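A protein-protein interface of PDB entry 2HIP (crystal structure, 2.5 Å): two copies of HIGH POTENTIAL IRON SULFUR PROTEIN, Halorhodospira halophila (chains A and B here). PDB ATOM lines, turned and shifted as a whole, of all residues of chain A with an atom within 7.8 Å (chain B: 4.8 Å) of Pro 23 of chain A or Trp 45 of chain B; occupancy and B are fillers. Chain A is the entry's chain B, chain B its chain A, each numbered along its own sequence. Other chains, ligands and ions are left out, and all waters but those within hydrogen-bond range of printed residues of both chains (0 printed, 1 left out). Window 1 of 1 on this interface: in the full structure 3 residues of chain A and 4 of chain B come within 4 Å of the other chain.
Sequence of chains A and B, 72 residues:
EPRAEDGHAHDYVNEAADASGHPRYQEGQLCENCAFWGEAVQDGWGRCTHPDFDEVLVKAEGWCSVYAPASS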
ATOM      1  N   ASP A  11      14.449   2.673  38.365  1.00  0.00           N
ATOM      2  CA  ASP A  11      14.096   4.021  38.020  1.00  0.00           C
ATOM      3  C   ASP A  11      12.597   4.232  37.747  1.00  0.00           C
ATOM      4  O   ASP A  11      12.222   5.113  36.976  1.00  0.00           O
ATOM      5  CB  ASP A  11      14.887   4.359  36.707  1.00  0.00           C
ATOM      6  CG  ASP A  11      16.400   4.538  36.845  1.00  0.00           C
ATOM      7  OD1 ASP A  11      16.915   5.157  37.759  1.00  0.00           O
ATOM      8  OD2 ASP A  11      17.089   3.977  35.871  1.00  0.00           O
ATOM      9  N   ALA A  19      10.438  10.085  33.179  1.00  0.00           N
ATOM     10  CA  ALA A  19      11.585   9.209  32.824  1.00  0.00           C
ATOM     11  C   ALA A  19      12.373   9.734  31.604  1.00  0.00           C
ATOM     12  O   ALA A  19      13.357   9.141  31.156  1.00  0.00           O
ATOM     13  CB  ALA A  19      11.094   7.788  32.574  1.00  0.00           C
ATOM     14  N   SER A  20      11.878  10.881  31.100  1.00  0.00           N
ATOM     15  CA  SER A  20      12.326  11.702  29.948  1.00  0.00           C
ATOM     16  C   SER A  20      13.806  11.682  29.570  1.00  0.00           C
ATOM     17  O   SER A  20      14.175  11.312  28.458  1.00  0.00           O
ATOM     18  CB  SER A  20      11.884  13.141  30.147  1.00  0.00           C
ATOM     19  OG  SER A  20      10.895  13.482  29.200  1.00  0.00           O
ATOM     20  N   GLY A  21      14.648  12.102  30.489  1.00  0.00           N
ATOM     21  CA  GLY A  21      16.062  12.135  30.222  1.00  0.00           C
ATOM     22  C   GLY A  21      16.751  10.801  30.453  1.00  0.00           C
ATOM     23  O   GLY A  21      17.897  10.756  30.886  1.00  0.00           O
ATOM     24  N   HIS A  22      16.053   9.712  30.173  1.00  0.00           N
ATOM     25  CA  HIS A  22      16.620   8.396  30.338  1.00  0.00           C
ATOM     26  C   HIS A  22      16.868   7.923  28.946  1.00  0.00           C
ATOM     27  O   HIS A  22      15.971   7.889  28.111  1.00  0.00           O
ATOM     28  CB  HIS A  22      15.725   7.434  31.153  1.00  0.00           C
ATOM     29  CG  HIS A  22      16.398   6.147  31.555  1.00  0.00           C
ATOM     30  ND1 HIS A  22      16.632   5.131  30.635  1.00  0.00           N
ATOM     31  CD2 HIS A  22      16.867   5.728  32.768  1.00  0.00           C
ATOM     32  CE1 HIS A  22      17.224   4.137  31.290  1.00  0.00           C
ATOM     33  NE2 HIS A  22      17.378   4.462  32.572  1.00  0.00           N
ATOM     34  N   PRO A  23      18.093   7.594  28.707  1.00  0.00           N
ATOM     35  CA  PRO A  23      18.564   7.149  27.433  1.00  0.00           C
ATOM     36  C   PRO A  23      17.728   6.121  26.728  1.00  0.00           C
ATOM     37  O   PRO A  23      17.598   6.143  25.508  1.00  0.00           O
ATOM     38  CB  PRO A  23      19.992   6.645  27.656  1.00  0.00           C
ATOM     39  CG  PRO A  23      20.256   6.692  29.156  1.00  0.00           C
ATOM     40  CD  PRO A  23      19.101   7.444  29.783  1.00  0.00           C
ATOM     41  N   ARG A  24      17.173   5.227  27.493  1.00  0.00           N
ATOM     42  CA  ARG A  24      16.370   4.174  26.950  1.00  0.00           C
ATOM     43  C   ARG A  24      14.930   4.562  26.685  1.00  0.00           C
ATOM     44  O   ARG A  24      14.244   3.945  25.871  1.00  0.00           O
ATOM     45  CB  ARG A  24      16.446   2.973  27.876  1.00  0.00           C
ATOM     46  CG  ARG A  24      16.293   1.645  27.162  1.00  0.00           C
ATOM     47  CD  ARG A  24      16.441   0.432  28.085  1.00  0.00           C
ATOM     48  NE  ARG A  24      16.002  -0.801  27.424  1.00  0.00           N
ATOM     49  CZ  ARG A  24      15.278  -1.794  27.966  1.00  0.00           C
ATOM     50  NH1 ARG A  24      14.862  -1.775  29.227  1.00  0.00           N
ATOM     51  NH2 ARG A  24      14.966  -2.844  27.208  1.00  0.00           N
ATOM     52  N   TYR A  25      14.484   5.585  27.384  1.00  0.00           N
ATOM     53  CA  TYR A  25      13.134   6.079  27.265  1.00  0.00           C
ATOM     54  C   TYR A  25      12.773   6.593  25.889  1.00  0.00           C
ATOM     55  O   TYR A  25      13.524   7.339  25.269  1.00  0.00           O
ATOM     56  CB  TYR A  25      12.883   7.222  28.262  1.00  0.00           C
ATOM     57  CG  TYR A  25      11.522   7.842  28.054  1.00  0.00           C
ATOM     58  CD1 TYR A  25      10.390   7.223  28.582  1.00  0.00           C
ATOM     59  CD2 TYR A  25      11.351   9.025  27.329  1.00  0.00           C
ATOM     60  CE1 TYR A  25       9.121   7.766  28.395  1.00  0.00           C
ATOM     61  CE2 TYR A  25      10.087   9.588  27.135  1.00  0.00           C
ATOM     62  CZ  TYR A  25       8.968   8.950  27.672  1.00  0.00           C
ATOM     63  OH  TYR A  25       7.714   9.482  27.500  1.00  0.00           O
ATOM     64  N   GLN A  26      11.600   6.209  25.423  1.00  0.00           N
ATOM     65  CA  GLN A  26      11.104   6.654  24.136  1.00  0.00           C
ATOM     66  C   GLN A  26       9.652   7.116  24.352  1.00  0.00           C
ATOM     67  O   GLN A  26       8.979   6.571  25.221  1.00  0.00           O
ATOM     68  CB  GLN A  26      11.218   5.557  23.028  1.00  0.00           C
ATOM     69  CG  GLN A  26      12.683   5.271  22.600  1.00  0.00           C
ATOM     70  CD  GLN A  26      12.868   4.242  21.477  1.00  0.00           C
ATOM     71  OE1 GLN A  26      12.031   4.108  20.572  1.00  0.00           O
ATOM     72  NE2 GLN A  26      13.993   3.528  21.528  1.00  0.00           N
ATOM     73  N   GLN A  29       6.110   4.833  25.342  1.00  0.00           N
ATOM     74  CA  GLN A  29       6.458   3.755  26.204  1.00  0.00           C
ATOM     75  C   GLN A  29       5.842   3.992  27.576  1.00  0.00           C
ATOM     76  O   GLN A  29       6.220   4.915  28.297  1.00  0.00           O
ATOM     77  CB  GLN A  29       7.980   3.592  26.318  1.00  0.00           C
ATOM     78  CG  GLN A  29       8.645   2.858  25.137  1.00  0.00           C
ATOM     79  CD  GLN A  29      10.160   2.859  25.259  1.00  0.00           C
ATOM     80  OE1 GLN A  29      10.720   3.377  26.240  1.00  0.00           O
ATOM     81  NE2 GLN A  29      10.830   2.290  24.264  1.00  0.00           N
ATOM     82  N   TRP A  63       6.466   4.157  33.902  1.00  0.00           N
ATOM     83  CA  TRP A  63       7.530   3.522  33.154  1.00  0.00           C
ATOM     84  C   TRP A  63       8.700   3.143  34.048  1.00  0.00           C
ATOM     85  O   TRP A  63       8.911   3.723  35.114  1.00  0.00           O
ATOM     86  CB  TRP A  63       8.051   4.548  32.080  1.00  0.00           C
ATOM     87  CG  TRP A  63       9.129   4.122  31.073  1.00  0.00           C
ATOM     88  CD1 TRP A  63       8.891   3.646  29.825  1.00  0.00           C
ATOM     89  CD2 TRP A  63      10.588   4.189  31.183  1.00  0.00           C
ATOM     90  NE1 TRP A  63      10.064   3.383  29.159  1.00  0.00           N
ATOM     91  CE2 TRP A  63      11.125   3.707  29.954  1.00  0.00           C
ATOM     92  CE3 TRP A  63      11.480   4.572  32.193  1.00  0.00           C
ATOM     93  CZ2 TRP A  63      12.502   3.613  29.721  1.00  0.00           C
ATOM     94  CZ3 TRP A  63      12.840   4.463  31.966  1.00  0.00           C
ATOM     95  CH2 TRP A  63      13.341   3.999  30.740  1.00  0.00           C
ATOM     96  N   ARG B   3      23.523   1.501  28.088  1.00  0.00           N
ATOM     97  CA  ARG B   3      24.429   2.251  28.893  1.00  0.00           C
ATOM     98  C   ARG B   3      25.522   1.331  29.372  1.00  0.00           C
ATOM     99  O   ARG B   3      25.333   0.121  29.530  1.00  0.00           O
ATOM    100  CB  ARG B   3      23.723   2.789  30.138  1.00  0.00           C
ATOM    101  CG  ARG B   3      22.898   4.069  29.992  1.00  0.00           C
ATOM    102  CD  ARG B   3      22.110   4.380  31.282  1.00  0.00           C
ATOM    103  NE  ARG B   3      21.159   3.312  31.634  1.00  0.00           N
ATOM    104  CZ  ARG B   3      20.575   3.104  32.829  1.00  0.00           C
ATOM    105  NH1 ARG B   3      20.800   3.880  33.890  1.00  0.00           N
ATOM    106  NH2 ARG B   3      19.735   2.076  32.951  1.00  0.00           N
ATOM    107  N   ALA B   4      26.657   1.913  29.618  1.00  0.00           N
ATOM    108  CA  ALA B   4      27.764   1.138  30.077  1.00  0.00           C
ATOM    109  C   ALA B   4      27.849   1.050  31.599  1.00  0.00           C
ATOM    110  O   ALA B   4      27.929   2.082  32.274  1.00  0.00           O
ATOM    111  CB  ALA B   4      29.051   1.706  29.500  1.00  0.00           C
ATOM    112  N   ASN B  14      31.192   5.400  35.697  1.00  0.00           N
ATOM    113  CA  ASN B  14      30.258   6.348  35.164  1.00  0.00           C
ATOM    114  C   ASN B  14      30.394   7.698  35.853  1.00  0.00           C
ATOM    115  O   ASN B  14      29.861   8.677  35.376  1.00  0.00           O
ATOM    116  CB  ASN B  14      28.834   5.844  35.268  1.00  0.00           C
ATOM    117  CG  ASN B  14      28.446   5.045  34.058  1.00  0.00           C
ATOM    118  OD1 ASN B  14      28.322   5.588  32.951  1.00  0.00           O
ATOM    119  ND2 ASN B  14      28.263   3.746  34.256  1.00  0.00           N
ATOM    120  N   TRP B  37      35.961  10.127  22.451  1.00  0.00           N
ATOM    121  CA  TRP B  37      34.589  10.626  22.519  1.00  0.00           C
ATOM    122  C   TRP B  37      33.988  11.013  21.174  1.00  0.00           C
ATOM    123  O   TRP B  37      34.532  11.834  20.434  1.00  0.00           O
ATOM    124  CB  TRP B  37      34.575  11.812  23.460  1.00  0.00           C
ATOM    125  CG  TRP B  37      33.302  12.547  23.644  1.00  0.00           C
ATOM    126  CD1 TRP B  37      33.046  13.784  23.168  1.00  0.00           C
ATOM    127  CD2 TRP B  37      32.174  12.154  24.414  1.00  0.00           C
ATOM    128  NE1 TRP B  37      31.811  14.186  23.564  1.00  0.00           N
ATOM    129  CE2 TRP B  37      31.256  13.202  24.336  1.00  0.00           C
ATOM    130  CE3 TRP B  37      31.857  11.013  25.152  1.00  0.00           C
ATOM    131  CZ2 TRP B  37      30.027  13.127  24.969  1.00  0.00           C
ATOM    132  CZ3 TRP B  37      30.643  10.938  25.781  1.00  0.00           C
ATOM    133  CH2 TRP B  37      29.738  11.987  25.688  1.00  0.00           C
ATOM    134  N   GLU B  39      30.831  12.331  20.870  1.00  0.00           N
ATOM    135  CA  GLU B  39      29.717  13.231  21.201  1.00  0.00           C
ATOM    136  C   GLU B  39      28.465  12.554  21.731  1.00  0.00           C
ATOM    137  O   GLU B  39      28.292  11.348  21.569  1.00  0.00           O
ATOM    138  CB  GLU B  39      29.329  14.083  20.016  1.00  0.00           C
ATOM    139  CG  GLU B  39      30.160  15.342  19.997  1.00  0.00           C
ATOM    140  CD  GLU B  39      30.251  15.942  18.649  1.00  0.00           C
ATOM    141  OE1 GLU B  39      29.824  15.152  17.691  1.00  0.00           O
ATOM    142  OE2 GLU B  39      30.687  17.055  18.471  1.00  0.00           O
ATOM    143  N   ALA B  40      27.580  13.385  22.360  1.00  0.00           N
ATOM    144  CA  ALA B  40      26.291  12.984  22.955  1.00  0.00           C
ATOM    145  C   ALA B  40      25.277  12.558  21.913  1.00  0.00           C
ATOM    146  O   ALA B  40      24.967  13.278  20.967  1.00  0.00           O
ATOM    147  CB  ALA B  40      25.725  14.075  23.856  1.00  0.00           C
ATOM    148  N   VAL B  41      24.782  11.365  22.126  1.00  0.00           N
ATOM    149  CA  VAL B  41      23.812  10.702  21.290  1.00  0.00           C
ATOM    150  C   VAL B  41      22.432  10.899  21.869  1.00  0.00           C
ATOM    151  O   VAL B  41      21.401  11.004  21.196  1.00  0.00           O
ATOM    152  CB  VAL B  41      24.195   9.243  21.346  1.00  0.00           C
ATOM    153  CG1 VAL B  41      22.974   8.354  21.216  1.00  0.00           C
ATOM    154  CG2 VAL B  41      25.207   8.933  20.258  1.00  0.00           C
ATOM    155  N   GLN B  42      22.498  10.931  23.159  1.00  0.00           N
ATOM    156  CA  GLN B  42      21.429  11.131  24.043  1.00  0.00           C
ATOM    157  C   GLN B  42      22.000  12.087  25.060  1.00  0.00           C
ATOM    158  O   GLN B  42      23.199  12.380  25.076  1.00  0.00           O
ATOM    159  CB  GLN B  42      20.900   9.825  24.712  1.00  0.00           C
ATOM    160  CG  GLN B  42      20.395   8.752  23.711  1.00  0.00           C
ATOM    161  CD  GLN B  42      18.879   8.664  23.578  1.00  0.00           C
ATOM    162  OE1 GLN B  42      18.359   8.113  22.594  1.00  0.00           O
ATOM    163  NE2 GLN B  42      18.170   9.195  24.570  1.00  0.00           N
ATOM    164  N   ASP B  43      21.115  12.562  25.869  1.00  0.00           N
ATOM    165  CA  ASP B  43      21.305  13.501  26.935  1.00  0.00           C
ATOM    166  C   ASP B  43      22.288  13.110  28.062  1.00  0.00           C
ATOM    167  O   ASP B  43      21.867  12.495  29.035  1.00  0.00           O
ATOM    168  CB  ASP B  43      19.881  13.709  27.510  1.00  0.00           C
ATOM    169  CG  ASP B  43      18.782  12.959  26.743  1.00  0.00           C
ATOM    170  OD1 ASP B  43      18.635  11.712  27.125  1.00  0.00           O
ATOM    171  OD2 ASP B  43      18.093  13.481  25.880  1.00  0.00           O
ATOM    172  N   GLY B  44      23.587  13.469  27.954  1.00  0.00           N
ATOM    173  CA  GLY B  44      24.577  13.136  29.001  1.00  0.00           C
ATOM    174  C   GLY B  44      25.348  11.840  28.719  1.00  0.00           C
ATOM    175  O   GLY B  44      26.280  11.468  29.440  1.00  0.00           O
ATOM    176  N   TRP B  45      24.925  11.169  27.638  1.00  0.00           N
ATOM    177  CA  TRP B  45      25.487   9.904  27.153  1.00  0.00           C
ATOM    178  C   TRP B  45      25.919   9.957  25.680  1.00  0.00           C
ATOM    179  O   TRP B  45      25.153  10.395  24.823  1.00  0.00           O
ATOM    180  CB  TRP B  45      24.466   8.771  27.326  1.00  0.00           C
ATOM    181  CG  TRP B  45      24.081   8.615  28.743  1.00  0.00           C
ATOM    182  CD1 TRP B  45      23.233   9.427  29.404  1.00  0.00           C
ATOM    183  CD2 TRP B  45      24.528   7.621  29.694  1.00  0.00           C
ATOM    184  NE1 TRP B  45      23.102   9.020  30.693  1.00  0.00           N
ATOM    185  CE2 TRP B  45      23.880   7.918  30.900  1.00  0.00           C
ATOM    186  CE3 TRP B  45      25.395   6.511  29.661  1.00  0.00           C
ATOM    187  CZ2 TRP B  45      24.071   7.155  32.055  1.00  0.00           C
ATOM    188  CZ3 TRP B  45      25.582   5.753  30.811  1.00  0.00           C
ATOM    189  CH2 TRP B  45      24.924   6.076  31.996  1.00  0.00           C
ATOM    190  N   GLY B  46      27.155   9.488  25.384  1.00  0.00           N
ATOM    191  CA  GLY B  46      27.671   9.492  24.003  1.00  0.00           C
ATOM    192  C   GLY B  46      28.397   8.211  23.542  1.00  0.00           C
ATOM    193  O   GLY B  46      28.423   7.196  24.241  1.00  0.00           O
ATOM    194  N   LEU B  57      26.880   2.762  25.376  1.00  0.00           N
ATOM    195  CA  LEU B  57      26.896   4.192  25.483  1.00  0.00           C
ATOM    196  C   LEU B  57      27.787   4.450  26.671  1.00  0.00           C
ATOM    197  O   LEU B  57      27.831   3.649  27.606  1.00  0.00           O
ATOM    198  CB  LEU B  57      25.496   4.792  25.823  1.00  0.00           C
ATOM    199  CG  LEU B  57      24.828   5.667  24.751  1.00  0.00           C
ATOM    200  CD1 LEU B  57      25.439   5.392  23.386  1.00  0.00           C
ATOM    201  CD2 LEU B  57      23.322   5.391  24.718  1.00  0.00           C
ATOM    202  N   VAL B  58      28.488   5.558  26.640  1.00  0.00           N
ATOM    203  CA  VAL B  58      29.362   5.949  27.726  1.00  0.00           C
ATOM    204  C   VAL B  58      28.799   7.267  28.295  1.00  0.00           C
ATOM    205  O   VAL B  58      28.012   7.929  27.623  1.00  0.00           O
ATOM    206  CB  VAL B  58      30.836   6.038  27.316  1.00  0.00           C
ATOM    207  CG1 VAL B  58      31.305   4.715  26.716  1.00  0.00           C
ATOM    208  CG2 VAL B  58      31.038   7.169  26.317  1.00  0.00           C
ATOM    209  N   LYS B  59      29.178   7.651  29.518  1.00  0.00           N
ATOM    210  CA  LYS B  59      28.669   8.873  30.153  1.00  0.00           C
ATOM    211  C   LYS B  59      29.625  10.062  30.194  1.00  0.00           C
ATOM    212  O   LYS B  59      30.764   9.937  30.635  1.00  0.00           O
ATOM    213  CB  LYS B  59      28.292   8.518  31.557  1.00  0.00           C
ATOM    214  CG  LYS B  59      27.845   9.703  32.352  1.00  0.00           C
ATOM    215  CD  LYS B  59      26.358   9.643  32.576  1.00  0.00           C
ATOM    216  CE  LYS B  59      25.974  10.065  33.972  1.00  0.00           C
ATOM    217  NZ  LYS B  59      26.192  11.497  34.192  1.00  0.00           N
ATOM    218  N   ALA B  60      29.130  11.217  29.743  1.00  0.00           N
ATOM    219  CA  ALA B  60      29.904  12.443  29.713  1.00  0.00           C
ATOM    220  C   ALA B  60      30.814  12.638  30.917  1.00  0.00           C
ATOM    221  O   ALA B  60      31.941  13.105  30.764  1.00  0.00           O
ATOM    222  CB  ALA B  60      29.049  13.670  29.418  1.00  0.00           C
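The guanidinium group (NH2) of Arg 3 of chain B sits at hydrogen-bond distance from a ring nitrogen (NE2) of His 22 of chain A (3.4 Å).
The side-chain amide nitrogen of Gln 42 of chain B sits at hydrogen-bond distance from the backbone carbonyl oxygen of Pro 23 of chain A (3.2 Å).
Asp 11 of chain A touches none of the printed residues of chain B.
Of the printed residues of chain B, Gly 21 of chain A touches Asp 43.
Of the printed residues of chain B, His 22 of chain A touches Arg 3.
Of the printed residues of chain B, Pro 23 of chain A touches Arg 3 (3.6 Å), Gln 42 (3.2 Å) and Trp 45 (3.99 Å).
Printed residues of chain A within 4 Å of Arg 3 of chain B: His 22 (3.4 Å) and Pro 23 (3.6 Å).
Printed residues of chain A within 4 Å of Gln 42 of chain B: Pro 23.
Of the printed residues of chain A, Asp 43 of chain B touches Gly 21.
Printed residues of chain A within 4 Å of Trp 45 of chain B: Pro 23.
Leu 57 of chain B touches none of the printed residues of chain A.
The nearest printed residue of chain A that does not touch Trp 45 of chain B is Gly 21 of chain A (5.5 Å).
The nearest printed residue of chain B that does not touch His 22 of chain A is Gln 42 of chain B (4.4 Å).
OD2 of Asp 11 of chain A lies within hydrogen-bond range of NE2 of His 22 of chain A (3.3 Å).
A ring nitrogen (ND1) of His 22 of chain A sits close to the backbone NH of Arg 24 of chain A, at 3.2 Å.
Hydrophobic or aromatic side chains of chain A that line the printed part of chain B: His 22 and Pro 23.
Of the 16 printed residues of chain B, 4 touch a printed residue of chain A.
Printed residues of chain B that touch a printed residue of chain A: Arg 3, Gln 42, Asp 43 and Trp 45.
Among the printed residues, 5 pairs touch across the chains.
No position is printed for both chains.
C of Gly 21 of chain A touches OD1 of Asp 43 of chain B, at 3.9 Å.
Pro 23 of chain A touches Arg 3 of chain B (CG to CD, 3.6 Å).
NE1 of Trp 45 of chain B touches CG of Pro 23 of chain A, 3.99 Å away.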
